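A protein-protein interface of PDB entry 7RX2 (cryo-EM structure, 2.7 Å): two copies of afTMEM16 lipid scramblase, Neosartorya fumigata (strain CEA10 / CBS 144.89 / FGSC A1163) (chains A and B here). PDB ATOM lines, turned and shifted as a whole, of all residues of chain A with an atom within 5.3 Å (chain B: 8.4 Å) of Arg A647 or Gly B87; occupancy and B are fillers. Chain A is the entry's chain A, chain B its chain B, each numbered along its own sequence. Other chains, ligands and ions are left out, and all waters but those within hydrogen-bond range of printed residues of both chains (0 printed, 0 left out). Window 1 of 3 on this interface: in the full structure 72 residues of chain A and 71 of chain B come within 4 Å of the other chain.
OD1 of Asn B90 sits at hydrogen-bond distance from NH1 of Arg A651 (2.8 Å). NH1 of Arg B651 sits at hydrogen-bond distance from OD1 of Asn A90 (2.8 Å). NH2 of Arg A651 sits close to O of Trp B84, 2.4 Å away.
The backbone carbonyl oxygen (O) of Glu B643 sits at hydrogen-bond distance from the side-chain amide nitrogen (ND2) of Asn B90 (2.7 Å). O of Glu A643 sits at hydrogen-bond distance from ND2 of Asn A90, at 2.7 Å.
Among the printed residues, merely in contact across the chains: Phe A648 with Leu B85 (3.2 Å), Met A650 with Arg B651 (3.2 Å), Arg A651 with Met B650 (3.4 Å), Arg A651 with Gly B87 (3.6 Å), Phe A648 with Tyr B86 (3.7 Å), Arg A647 with Tyr B86 (3.7 Å), Arg A647 with Gly B87 (3.7 Å) and Arg A651 with Leu B85 (3.8 Å).
Of the printed residues of chain B, Asn A90 touches Arg B651 (2.8 Å). Glu A646 touches none of the printed residues of chain B. Printed residues of chain B within 4 Å of Phe A648: Leu B85 and Tyr B86. Of the printed residues of chain B, Met A650 touches Arg B651 (3.2 Å). Of the printed residues of chain B, Arg A651 touches Trp B84 (2.4 Å), Leu B85 (3.8 Å), Gly B87 (3.6 Å), Asn B90 (2.8 Å) and Met B650 (3.4 Å). Of the printed residues of chain A, Tyr B86 touches Arg A647 and Phe A648. Of chain A, only Arg A647 and Arg A651 come within 4 Å of Gly B87. The nearest printed residue of chain A that does not touch Gly B87 is Phe A648 (6.3 Å). The nearest printed residue of chain A that does not touch Asn B90 is Arg A647 (5.5 Å).
Hydrophobic or aromatic side chains of chain A that line the printed part of chain B: Phe A648 and Met A650. Of the 23 printed residues of chain B, 7 touch a printed residue of chain A. Among the printed residues, no Asp or Glu carboxylate lies within 4 Å of a Lys or Arg side-chain nitrogen of the other chain.
Asn A90 touches Arg B651, and with the chains exchanged Arg A651 touches Asn B90. Met A650 touches Arg B651, and with the chains exchanged Arg A651 touches Met B650. 5 positions are printed for both chains.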
ATOM      1  N   ASN A  90       9.470  15.400 -18.003  1.00  0.00           N
ATOM      2  CA  ASN A  90       9.128  15.136 -19.397  1.00  0.00           C
ATOM      3  C   ASN A  90       9.431  13.717 -19.856  1.00  0.00           C
ATOM      4  O   ASN A  90       9.057  13.360 -20.963  1.00  0.00           O
ATOM      5  CB  ASN A  90       9.831  16.106 -20.352  1.00  0.00           C
ATOM      6  CG  ASN A  90       8.924  16.632 -21.394  1.00  0.00           C
ATOM      7  OD1 ASN A  90       7.757  16.270 -21.444  1.00  0.00           O
ATOM      8  ND2 ASN A  90       9.438  17.516 -22.231  1.00  0.00           N
ATOM      9  N   ARG A 642      16.149  18.283 -27.096  1.00  0.00           N
ATOM     10  CA  ARG A 642      15.907  16.904 -26.707  1.00  0.00           C
ATOM     11  C   ARG A 642      14.727  16.784 -25.754  1.00  0.00           C
ATOM     12  O   ARG A 642      14.069  15.740 -25.721  1.00  0.00           O
ATOM     13  CB  ARG A 642      17.173  16.325 -26.093  1.00  0.00           C
ATOM     14  CG  ARG A 642      17.086  14.887 -25.690  1.00  0.00           C
ATOM     15  CD  ARG A 642      18.011  14.643 -24.535  1.00  0.00           C
ATOM     16  NE  ARG A 642      17.658  15.512 -23.419  1.00  0.00           N
ATOM     17  CZ  ARG A 642      18.492  15.889 -22.458  1.00  0.00           C
ATOM     18  NH1 ARG A 642      18.061  16.683 -21.493  1.00  0.00           N
ATOM     19  NH2 ARG A 642      19.751  15.473 -22.461  1.00  0.00           N
ATOM     20  N   GLU A 643      14.443  17.823 -24.968  1.00  0.00           N
ATOM     21  CA  GLU A 643      13.251  17.816 -24.132  1.00  0.00           C
ATOM     22  C   GLU A 643      11.988  18.110 -24.922  1.00  0.00           C
ATOM     23  O   GLU A 643      10.914  17.649 -24.534  1.00  0.00           O
ATOM     24  CB  GLU A 643      13.371  18.828 -22.989  1.00  0.00           C
ATOM     25  CG  GLU A 643      14.482  18.550 -21.994  1.00  0.00           C
ATOM     26  CD  GLU A 643      14.468  17.130 -21.447  1.00  0.00           C
ATOM     27  OE1 GLU A 643      13.435  16.699 -20.894  1.00  0.00           O
ATOM     28  OE2 GLU A 643      15.496  16.440 -21.571  1.00  0.00           O
ATOM     29  N   ARG A 644      12.088  18.868 -26.012  1.00  0.00           N
ATOM     30  CA  ARG A 644      10.928  19.065 -26.873  1.00  0.00           C
ATOM     31  C   ARG A 644      10.587  17.791 -27.626  1.00  0.00           C
ATOM     32  O   ARG A 644       9.413  17.444 -27.766  1.00  0.00           O
ATOM     33  CB  ARG A 644      11.186  20.210 -27.849  1.00  0.00           C
ATOM     34  CG  ARG A 644      10.096  20.392 -28.880  1.00  0.00           C
ATOM     35  CD  ARG A 644      10.294  21.630 -29.729  1.00  0.00           C
ATOM     36  NE  ARG A 644      11.548  21.614 -30.470  1.00  0.00           N
ATOM     37  CZ  ARG A 644      11.787  20.842 -31.523  1.00  0.00           C
ATOM     38  NH1 ARG A 644      10.858  20.009 -31.964  1.00  0.00           N
ATOM     39  NH2 ARG A 644      12.959  20.897 -32.133  1.00  0.00           N
ATOM     40  N   ILE A 645      11.599  17.085 -28.121  1.00  0.00           N
ATOM     41  CA  ILE A 645      11.355  15.807 -28.774  1.00  0.00           C
ATOM     42  C   ILE A 645      10.822  14.790 -27.777  1.00  0.00           C
ATOM     43  O   ILE A 645       9.967  13.967 -28.110  1.00  0.00           O
ATOM     44  CB  ILE A 645      12.638  15.300 -29.451  1.00  0.00           C
ATOM     45  CG1 ILE A 645      13.104  16.284 -30.523  1.00  0.00           C
ATOM     46  CG2 ILE A 645      12.422  13.922 -30.019  1.00  0.00           C
ATOM     47  CD1 ILE A 645      12.009  16.805 -31.389  1.00  0.00           C
ATOM     48  N   GLU A 646      11.317  14.827 -26.542  1.00  0.00           N
ATOM     49  CA  GLU A 646      10.931  13.814 -25.570  1.00  0.00           C
ATOM     50  C   GLU A 646       9.506  14.014 -25.074  1.00  0.00           C
ATOM     51  O   GLU A 646       8.854  13.048 -24.671  1.00  0.00           O
ATOM     52  CB  GLU A 646      11.909  13.805 -24.403  1.00  0.00           C
ATOM     53  CG  GLU A 646      11.449  12.978 -23.225  1.00  0.00           C
ATOM     54  CD  GLU A 646      11.507  11.487 -23.485  1.00  0.00           C
ATOM     55  OE1 GLU A 646      12.526  11.008 -24.020  1.00  0.00           O
ATOM     56  OE2 GLU A 646      10.531  10.787 -23.153  1.00  0.00           O
ATOM     57  N   ARG A 647       9.000  15.245 -25.090  1.00  0.00           N
ATOM     58  CA  ARG A 647       7.594  15.436 -24.766  1.00  0.00           C
ATOM     59  C   ARG A 647       6.693  14.892 -25.862  1.00  0.00           C
ATOM     60  O   ARG A 647       5.596  14.409 -25.575  1.00  0.00           O
ATOM     61  CB  ARG A 647       7.294  16.905 -24.524  1.00  0.00           C
ATOM     62  CG  ARG A 647       5.943  17.132 -23.901  1.00  0.00           C
ATOM     63  CD  ARG A 647       5.729  18.584 -23.573  1.00  0.00           C
ATOM     64  NE  ARG A 647       5.669  19.393 -24.784  1.00  0.00           N
ATOM     65  CZ  ARG A 647       4.579  20.011 -25.224  1.00  0.00           C
ATOM     66  NH1 ARG A 647       4.629  20.723 -26.339  1.00  0.00           N
ATOM     67  NH2 ARG A 647       3.446  19.928 -24.548  1.00  0.00           N
ATOM     68  N   PHE A 648       7.131  14.965 -27.115  1.00  0.00           N
ATOM     69  CA  PHE A 648       6.375  14.361 -28.203  1.00  0.00           C
ATOM     70  C   PHE A 648       6.351  12.849 -28.063  1.00  0.00           C
ATOM     71  O   PHE A 648       5.291  12.226 -28.142  1.00  0.00           O
ATOM     72  CB  PHE A 648       6.976  14.782 -29.547  1.00  0.00           C
ATOM     73  CG  PHE A 648       6.375  14.089 -30.734  1.00  0.00           C
ATOM     74  CD1 PHE A 648       5.270  14.611 -31.363  1.00  0.00           C
ATOM     75  CD2 PHE A 648       6.934  12.929 -31.240  1.00  0.00           C
ATOM     76  CE1 PHE A 648       4.718  13.978 -32.453  1.00  0.00           C
ATOM     77  CE2 PHE A 648       6.379  12.295 -32.324  1.00  0.00           C
ATOM     78  CZ  PHE A 648       5.272  12.824 -32.931  1.00  0.00           C
ATOM     79  N   MET A 649       7.519  12.239 -27.853  1.00  0.00           N
ATOM     80  CA  MET A 649       7.613  10.791 -27.763  1.00  0.00           C
ATOM     81  C   MET A 649       6.911  10.233 -26.540  1.00  0.00           C
ATOM     82  O   MET A 649       6.486   9.078 -26.566  1.00  0.00           O
ATOM     83  CB  MET A 649       9.075  10.359 -27.756  1.00  0.00           C
ATOM     84  CG  MET A 649       9.784  10.570 -29.070  1.00  0.00           C
ATOM     85  SD  MET A 649       8.888   9.874 -30.466  1.00  0.00           S
ATOM     86  CE  MET A 649       8.726   8.162 -29.966  1.00  0.00           C
ATOM     87  N   MET A 650       6.789  11.012 -25.466  1.00  0.00           N
ATOM     88  CA  MET A 650       5.997  10.564 -24.330  1.00  0.00           C
ATOM     89  C   MET A 650       4.529  10.465 -24.703  1.00  0.00           C
ATOM     90  O   MET A 650       3.859   9.487 -24.357  1.00  0.00           O
ATOM     91  CB  MET A 650       6.180  11.515 -23.152  1.00  0.00           C
ATOM     92  CG  MET A 650       5.536  11.050 -21.874  1.00  0.00           C
ATOM     93  SD  MET A 650       3.864  11.665 -21.645  1.00  0.00           S
ATOM     94  CE  MET A 650       4.189  13.372 -21.266  1.00  0.00           C
ATOM     95  N   ARG A 651       4.008  11.474 -25.393  1.00  0.00           N
ATOM     96  CA  ARG A 651       2.616  11.440 -25.804  1.00  0.00           C
ATOM     97  C   ARG A 651       2.369  10.348 -26.830  1.00  0.00           C
ATOM     98  O   ARG A 651       1.264   9.810 -26.903  1.00  0.00           O
ATOM     99  CB  ARG A 651       2.201  12.803 -26.345  1.00  0.00           C
ATOM    100  CG  ARG A 651       1.843  13.782 -25.266  1.00  0.00           C
ATOM    101  CD  ARG A 651       1.712  15.177 -25.780  1.00  0.00           C
ATOM    102  NE  ARG A 651       1.313  16.082 -24.715  1.00  0.00           N
ATOM    103  CZ  ARG A 651       0.346  16.981 -24.815  1.00  0.00           C
ATOM    104  NH1 ARG A 651       0.058  17.760 -23.793  1.00  0.00           N
ATOM    105  NH2 ARG A 651      -0.325  17.106 -25.940  1.00  0.00           N
ATOM    106  N   ARG B  80      -6.739  15.687 -35.037  1.00  0.00           N
ATOM    107  CA  ARG B  80      -6.713  15.964 -33.610  1.00  0.00           C
ATOM    108  C   ARG B  80      -5.588  15.217 -32.920  1.00  0.00           C
ATOM    109  O   ARG B  80      -5.055  15.690 -31.914  1.00  0.00           O
ATOM    110  CB  ARG B  80      -8.049  15.589 -32.988  1.00  0.00           C
ATOM    111  CG  ARG B  80      -9.185  16.439 -33.447  1.00  0.00           C
ATOM    112  CD  ARG B  80     -10.476  15.952 -32.870  1.00  0.00           C
ATOM    113  NE  ARG B  80     -11.602  16.734 -33.354  1.00  0.00           N
ATOM    114  CZ  ARG B  80     -12.871  16.389 -33.191  1.00  0.00           C
ATOM    115  NH1 ARG B  80     -13.178  15.272 -32.556  1.00  0.00           N
ATOM    116  NH2 ARG B  80     -13.828  17.160 -33.665  1.00  0.00           N
ATOM    117  N   VAL B  81      -5.226  14.045 -33.430  1.00  0.00           N
ATOM    118  CA  VAL B  81      -4.103  13.313 -32.868  1.00  0.00           C
ATOM    119  C   VAL B  81      -2.802  14.039 -33.155  1.00  0.00           C
ATOM    120  O   VAL B  81      -1.896  14.068 -32.317  1.00  0.00           O
ATOM    121  CB  VAL B  81      -4.084  11.879 -33.409  1.00  0.00           C
ATOM    122  CG1 VAL B  81      -2.711  11.288 -33.271  1.00  0.00           C
ATOM    123  CG2 VAL B  81      -5.089  11.050 -32.664  1.00  0.00           C
ATOM    124  N   ARG B  82      -2.686  14.644 -34.332  1.00  0.00           N
ATOM    125  CA  ARG B  82      -1.468  15.368 -34.657  1.00  0.00           C
ATOM    126  C   ARG B  82      -1.307  16.598 -33.777  1.00  0.00           C
ATOM    127  O   ARG B  82      -0.198  16.912 -33.346  1.00  0.00           O
ATOM    128  CB  ARG B  82      -1.458  15.751 -36.132  1.00  0.00           C
ATOM    129  CG  ARG B  82      -0.229  16.511 -36.540  1.00  0.00           C
ATOM    130  CD  ARG B  82      -0.019  16.482 -38.035  1.00  0.00           C
ATOM    131  NE  ARG B  82       0.382  17.785 -38.539  1.00  0.00           N
ATOM    132  CZ  ARG B  82       1.636  18.140 -38.784  1.00  0.00           C
ATOM    133  NH1 ARG B  82       2.621  17.281 -38.587  1.00  0.00           N
ATOM    134  NH2 ARG B  82       1.902  19.354 -39.239  1.00  0.00           N
ATOM    135  N   ASP B  83      -2.401  17.299 -33.491  1.00  0.00           N
ATOM    136  CA  ASP B  83      -2.324  18.439 -32.587  1.00  0.00           C
ATOM    137  C   ASP B  83      -1.928  18.010 -31.186  1.00  0.00           C
ATOM    138  O   ASP B  83      -1.076  18.641 -30.557  1.00  0.00           O
ATOM    139  CB  ASP B  83      -3.660  19.166 -32.537  1.00  0.00           C
ATOM    140  CG  ASP B  83      -3.866  20.075 -33.708  1.00  0.00           C
ATOM    141  OD1 ASP B  83      -2.957  20.165 -34.551  1.00  0.00           O
ATOM    142  OD2 ASP B  83      -4.938  20.700 -33.789  1.00  0.00           O
ATOM    143  N   TRP B  84      -2.548  16.950 -30.673  1.00  0.00           N
ATOM    144  CA  TRP B  84      -2.262  16.510 -29.317  1.00  0.00           C
ATOM    145  C   TRP B  84      -0.829  16.026 -29.176  1.00  0.00           C
ATOM    146  O   TRP B  84      -0.185  16.304 -28.164  1.00  0.00           O
ATOM    147  CB  TRP B  84      -3.250  15.421 -28.906  1.00  0.00           C
ATOM    148  CG  TRP B  84      -3.024  14.887 -27.534  1.00  0.00           C
ATOM    149  CD1 TRP B  84      -3.370  15.475 -26.366  1.00  0.00           C
ATOM    150  CD2 TRP B  84      -2.398  13.653 -27.190  1.00  0.00           C
ATOM    151  NE1 TRP B  84      -3.000  14.693 -25.313  1.00  0.00           N
ATOM    152  CE2 TRP B  84      -2.399  13.563 -25.794  1.00  0.00           C
ATOM    153  CE3 TRP B  84      -1.837  12.615 -27.929  1.00  0.00           C
ATOM    154  CZ2 TRP B  84      -1.864  12.481 -25.123  1.00  0.00           C
ATOM    155  CZ3 TRP B  84      -1.304  11.549 -27.261  1.00  0.00           C
ATOM    156  CH2 TRP B  84      -1.323  11.485 -25.875  1.00  0.00           C
ATOM    157  N   LEU B  85      -0.310  15.317 -30.175  1.00  0.00           N
ATOM    158  CA  LEU B  85       1.059  14.832 -30.098  1.00  0.00           C
ATOM    159  C   LEU B  85       2.058  15.972 -30.037  1.00  0.00           C
ATOM    160  O   LEU B  85       3.096  15.846 -29.387  1.00  0.00           O
ATOM    161  CB  LEU B  85       1.379  13.940 -31.291  1.00  0.00           C
ATOM    162  CG  LEU B  85       0.806  12.532 -31.331  1.00  0.00           C
ATOM    163  CD1 LEU B  85       1.243  11.844 -32.593  1.00  0.00           C
ATOM    164  CD2 LEU B  85       1.251  11.748 -30.138  1.00  0.00           C
ATOM    165  N   TYR B  86       1.774  17.083 -30.703  1.00  0.00           N
ATOM    166  CA  TYR B  86       2.699  18.201 -30.746  1.00  0.00           C
ATOM    167  C   TYR B  86       2.435  19.230 -29.663  1.00  0.00           C
ATOM    168  O   TYR B  86       3.097  20.269 -29.648  1.00  0.00           O
ATOM    169  CB  TYR B  86       2.656  18.864 -32.117  1.00  0.00           C
ATOM    170  CG  TYR B  86       3.425  18.089 -33.141  1.00  0.00           C
ATOM    171  CD1 TYR B  86       4.788  18.255 -33.276  1.00  0.00           C
ATOM    172  CD2 TYR B  86       2.796  17.166 -33.950  1.00  0.00           C
ATOM    173  CE1 TYR B  86       5.492  17.542 -34.197  1.00  0.00           C
ATOM    174  CE2 TYR B  86       3.489  16.448 -34.871  1.00  0.00           C
ATOM    175  CZ  TYR B  86       4.838  16.638 -34.994  1.00  0.00           C
ATOM    176  OH  TYR B  86       5.541  15.916 -35.922  1.00  0.00           O
ATOM    177  N   GLY B  87       1.497  18.970 -28.763  1.00  0.00           N
ATOM    178  CA  GLY B  87       1.281  19.838 -27.632  1.00  0.00           C
ATOM    179  C   GLY B  87       0.379  21.014 -27.883  1.00  0.00           C
ATOM    180  O   GLY B  87       0.342  21.933 -27.061  1.00  0.00           O
ATOM    181  N   VAL B  88      -0.354  21.020 -28.987  1.00  0.00           N
ATOM    182  CA  VAL B  88      -1.280  22.104 -29.272  1.00  0.00           C
ATOM    183  C   VAL B  88      -2.581  21.940 -28.498  1.00  0.00           C
ATOM    184  O   VAL B  88      -3.189  22.926 -28.087  1.00  0.00           O
ATOM    185  CB  VAL B  88      -1.530  22.184 -30.788  1.00  0.00           C
ATOM    186  CG1 VAL B  88      -2.493  23.294 -31.111  1.00  0.00           C
ATOM    187  CG2 VAL B  88      -0.238  22.378 -31.520  1.00  0.00           C
ATOM    188  N   ARG B  89      -3.026  20.706 -28.275  1.00  0.00           N
ATOM    189  CA  ARG B  89      -4.360  20.460 -27.739  1.00  0.00           C
ATOM    190  C   ARG B  89      -4.384  20.338 -26.225  1.00  0.00           C
ATOM    191  O   ARG B  89      -5.161  21.030 -25.561  1.00  0.00           O
ATOM    192  CB  ARG B  89      -4.946  19.194 -28.353  1.00  0.00           C
ATOM    193  CG  ARG B  89      -5.773  19.433 -29.570  1.00  0.00           C
ATOM    194  CD  ARG B  89      -6.348  18.131 -30.058  1.00  0.00           C
ATOM    195  NE  ARG B  89      -7.203  17.526 -29.051  1.00  0.00           N
ATOM    196  CZ  ARG B  89      -8.517  17.699 -29.005  1.00  0.00           C
ATOM    197  NH1 ARG B  89      -9.115  18.459 -29.912  1.00  0.00           N
ATOM    198  NH2 ARG B  89      -9.229  17.115 -28.054  1.00  0.00           N
ATOM    199  N   ASN B  90      -3.577  19.438 -25.673  1.00  0.00           N
ATOM    200  CA  ASN B  90      -3.421  19.178 -24.246  1.00  0.00           C
ATOM    201  C   ASN B  90      -4.532  18.333 -23.640  1.00  0.00           C
ATOM    202  O   ASN B  90      -4.421  17.950 -22.486  1.00  0.00           O
ATOM    203  CB  ASN B  90      -3.315  20.475 -23.438  1.00  0.00           C
ATOM    204  CG  ASN B  90      -2.237  20.426 -22.427  1.00  0.00           C
ATOM    205  OD1 ASN B  90      -1.558  19.418 -22.289  1.00  0.00           O
ATOM    206  ND2 ASN B  90      -2.043  21.524 -21.718  1.00  0.00           N
ATOM    207  N   THR B  91      -5.590  18.020 -24.374  1.00  0.00           N
ATOM    208  CA  THR B  91      -6.579  17.048 -23.932  1.00  0.00           C
ATOM    209  C   THR B  91      -6.588  15.898 -24.921  1.00  0.00           C
ATOM    210  O   THR B  91      -6.451  16.110 -26.127  1.00  0.00           O
ATOM    211  CB  THR B  91      -7.977  17.662 -23.829  1.00  0.00           C
ATOM    212  OG1 THR B  91      -8.914  16.666 -23.404  1.00  0.00           O
ATOM    213  CG2 THR B  91      -8.412  18.202 -25.172  1.00  0.00           C
ATOM    214  N   GLN B 239      -7.743  26.667 -28.646  1.00  0.00           N
ATOM    215  CA  GLN B 239      -6.915  25.474 -28.787  1.00  0.00           C
ATOM    216  C   GLN B 239      -5.908  25.618 -29.921  1.00  0.00           C
ATOM    217  O   GLN B 239      -5.632  24.669 -30.649  1.00  0.00           O
ATOM    218  CB  GLN B 239      -7.770  24.224 -28.987  1.00  0.00           C
ATOM    219  CG  GLN B 239      -8.881  24.051 -27.974  1.00  0.00           C
ATOM    220  CD  GLN B 239      -8.373  23.557 -26.642  1.00  0.00           C
ATOM    221  OE1 GLN B 239      -7.436  22.770 -26.581  1.00  0.00           O
ATOM    222  NE2 GLN B 239      -8.987  24.024 -25.564  1.00  0.00           N
ATOM    223  N   THR B 240      -5.338  26.805 -30.067  1.00  0.00           N
ATOM    224  CA  THR B 240      -4.299  27.048 -31.056  1.00  0.00           C
ATOM    225  C   THR B 240      -3.011  27.525 -30.407  1.00  0.00           C
ATOM    226  O   THR B 240      -2.180  28.142 -31.067  1.00  0.00           O
ATOM    227  CB  THR B 240      -4.754  28.065 -32.099  1.00  0.00           C
ATOM    228  OG1 THR B 240      -5.255  29.232 -31.443  1.00  0.00           O
ATOM    229  CG2 THR B 240      -5.824  27.488 -32.973  1.00  0.00           C
ATOM    230  N   LYS B 241      -2.831  27.221 -29.121  1.00  0.00           N
ATOM    231  CA  LYS B 241      -1.812  27.890 -28.318  1.00  0.00           C
ATOM    232  C   LYS B 241      -0.411  27.679 -28.878  1.00  0.00           C
ATOM    233  O   LYS B 241       0.305  28.647 -29.153  1.00  0.00           O
ATOM    234  CB  LYS B 241      -1.887  27.411 -26.876  1.00  0.00           C
ATOM    235  CG  LYS B 241      -0.870  28.061 -25.972  1.00  0.00           C
ATOM    236  CD  LYS B 241      -0.824  27.360 -24.628  1.00  0.00           C
ATOM    237  CE  LYS B 241       0.336  27.849 -23.789  1.00  0.00           C
ATOM    238  NZ  LYS B 241       0.180  29.282 -23.417  1.00  0.00           N
ATOM    239  N   GLY B 242       0.000  26.438 -29.066  1.00  0.00           N
ATOM    240  CA  GLY B 242       1.317  26.227 -29.632  1.00  0.00           C
ATOM    241  C   GLY B 242       1.271  25.843 -31.092  1.00  0.00           C
ATOM    242  O   GLY B 242       2.015  24.964 -31.527  1.00  0.00           O
ATOM    243  N   VAL B 243       0.402  26.496 -31.867  1.00  0.00           N
ATOM    244  CA  VAL B 243       0.086  26.020 -33.208  1.00  0.00           C
ATOM    245  C   VAL B 243       1.260  26.117 -34.165  1.00  0.00           C
ATOM    246  O   VAL B 243       1.219  25.509 -35.233  1.00  0.00           O
ATOM    247  CB  VAL B 243      -1.113  26.788 -33.796  1.00  0.00           C
ATOM    248  CG1 VAL B 243      -0.688  28.153 -34.291  1.00  0.00           C
ATOM    249  CG2 VAL B 243      -1.783  25.981 -34.882  1.00  0.00           C
ATOM    250  N   ALA B 245       3.988  24.696 -33.899  1.00  0.00           N
ATOM    251  CA  ALA B 245       4.657  23.409 -33.958  1.00  0.00           C
ATOM    252  C   ALA B 245       4.092  22.501 -35.037  1.00  0.00           C
ATOM    253  O   ALA B 245       4.733  21.508 -35.385  1.00  0.00           O
ATOM    254  CB  ALA B 245       4.566  22.717 -32.602  1.00  0.00           C
ATOM    255  N   VAL B 246       2.914  22.810 -35.569  1.00  0.00           N
ATOM    256  CA  VAL B 246       2.310  22.010 -36.628  1.00  0.00           C
ATOM    257  C   VAL B 246       2.077  22.879 -37.853  1.00  0.00           C
ATOM    258  O   VAL B 246       1.112  22.675 -38.596  1.00  0.00           O
ATOM    259  CB  VAL B 246       0.990  21.369 -36.168  1.00  0.00           C
ATOM    260  CG1 VAL B 246       1.224  20.449 -34.995  1.00  0.00           C
ATOM    261  CG2 VAL B 246      -0.014  22.435 -35.813  1.00  0.00           C
ATOM    262  N   GLU B 643      -5.615  25.230 -19.239  1.00  0.00           N
ATOM    263  CA  GLU B 643      -4.730  24.377 -20.019  1.00  0.00           C
ATOM    264  C   GLU B 643      -3.533  23.896 -19.217  1.00  0.00           C
ATOM    265  O   GLU B 643      -3.007  22.820 -19.507  1.00  0.00           O
ATOM    266  CB  GLU B 643      -4.232  25.099 -21.274  1.00  0.00           C
ATOM    267  CG  GLU B 643      -5.309  25.473 -22.276  1.00  0.00           C
ATOM    268  CD  GLU B 643      -6.216  24.311 -22.655  1.00  0.00           C
ATOM    269  OE1 GLU B 643      -5.711  23.266 -23.112  1.00  0.00           O
ATOM    270  OE2 GLU B 643      -7.444  24.445 -22.493  1.00  0.00           O
ATOM    271  N   ARG B 647      -3.019  19.831 -18.603  1.00  0.00           N
ATOM    272  CA  ARG B 647      -1.821  19.054 -18.889  1.00  0.00           C
ATOM    273  C   ARG B 647      -1.420  18.192 -17.703  1.00  0.00           C
ATOM    274  O   ARG B 647      -0.887  17.097 -17.889  1.00  0.00           O
ATOM    275  CB  ARG B 647      -0.672  19.964 -19.286  1.00  0.00           C
ATOM    276  CG  ARG B 647       0.493  19.215 -19.876  1.00  0.00           C
ATOM    277  CD  ARG B 647       1.560  20.158 -20.359  1.00  0.00           C
ATOM    278  NE  ARG B 647       2.166  20.879 -19.247  1.00  0.00           N
ATOM    279  CZ  ARG B 647       3.419  20.715 -18.837  1.00  0.00           C
ATOM    280  NH1 ARG B 647       3.876  21.421 -17.814  1.00  0.00           N
ATOM    281  NH2 ARG B 647       4.217  19.860 -19.454  1.00  0.00           N
ATOM    282  N   MET B 650      -3.958  15.231 -17.656  1.00  0.00           N
ATOM    283  CA  MET B 650      -3.674  14.257 -18.700  1.00  0.00           C
ATOM    284  C   MET B 650      -2.585  13.298 -18.260  1.00  0.00           C
ATOM    285  O   MET B 650      -2.696  12.085 -18.464  1.00  0.00           O
ATOM    286  CB  MET B 650      -3.266  14.968 -19.986  1.00  0.00           C
ATOM    287  CG  MET B 650      -3.112  14.060 -21.175  1.00  0.00           C
ATOM    288  SD  MET B 650      -1.439  13.451 -21.406  1.00  0.00           S
ATOM    289  CE  MET B 650      -0.629  14.923 -21.991  1.00  0.00           C
ATOM    290  N   ARG B 651      -1.515  13.823 -17.669  1.00  0.00           N
ATOM    291  CA  ARG B 651      -0.441  12.965 -17.202  1.00  0.00           C
ATOM    292  C   ARG B 651      -0.896  12.088 -16.049  1.00  0.00           C
ATOM    293  O   ARG B 651      -0.376  10.986 -15.870  1.00  0.00           O
ATOM    294  CB  ARG B 651       0.762  13.811 -16.804  1.00  0.00           C
ATOM    295  CG  ARG B 651       1.612  14.213 -17.973  1.00  0.00           C
ATOM    296  CD  ARG B 651       2.615  15.260 -17.617  1.00  0.00           C
ATOM    297  NE  ARG B 651       3.451  15.582 -18.762  1.00  0.00           N
ATOM    298  CZ  ARG B 651       4.771  15.673 -18.727  1.00  0.00           C
ATOM    299  NH1 ARG B 651       5.444  15.972 -19.819  1.00  0.00           N
ATOM    300  NH2 ARG B 651       5.417  15.473 -17.597  1.00  0.00           N
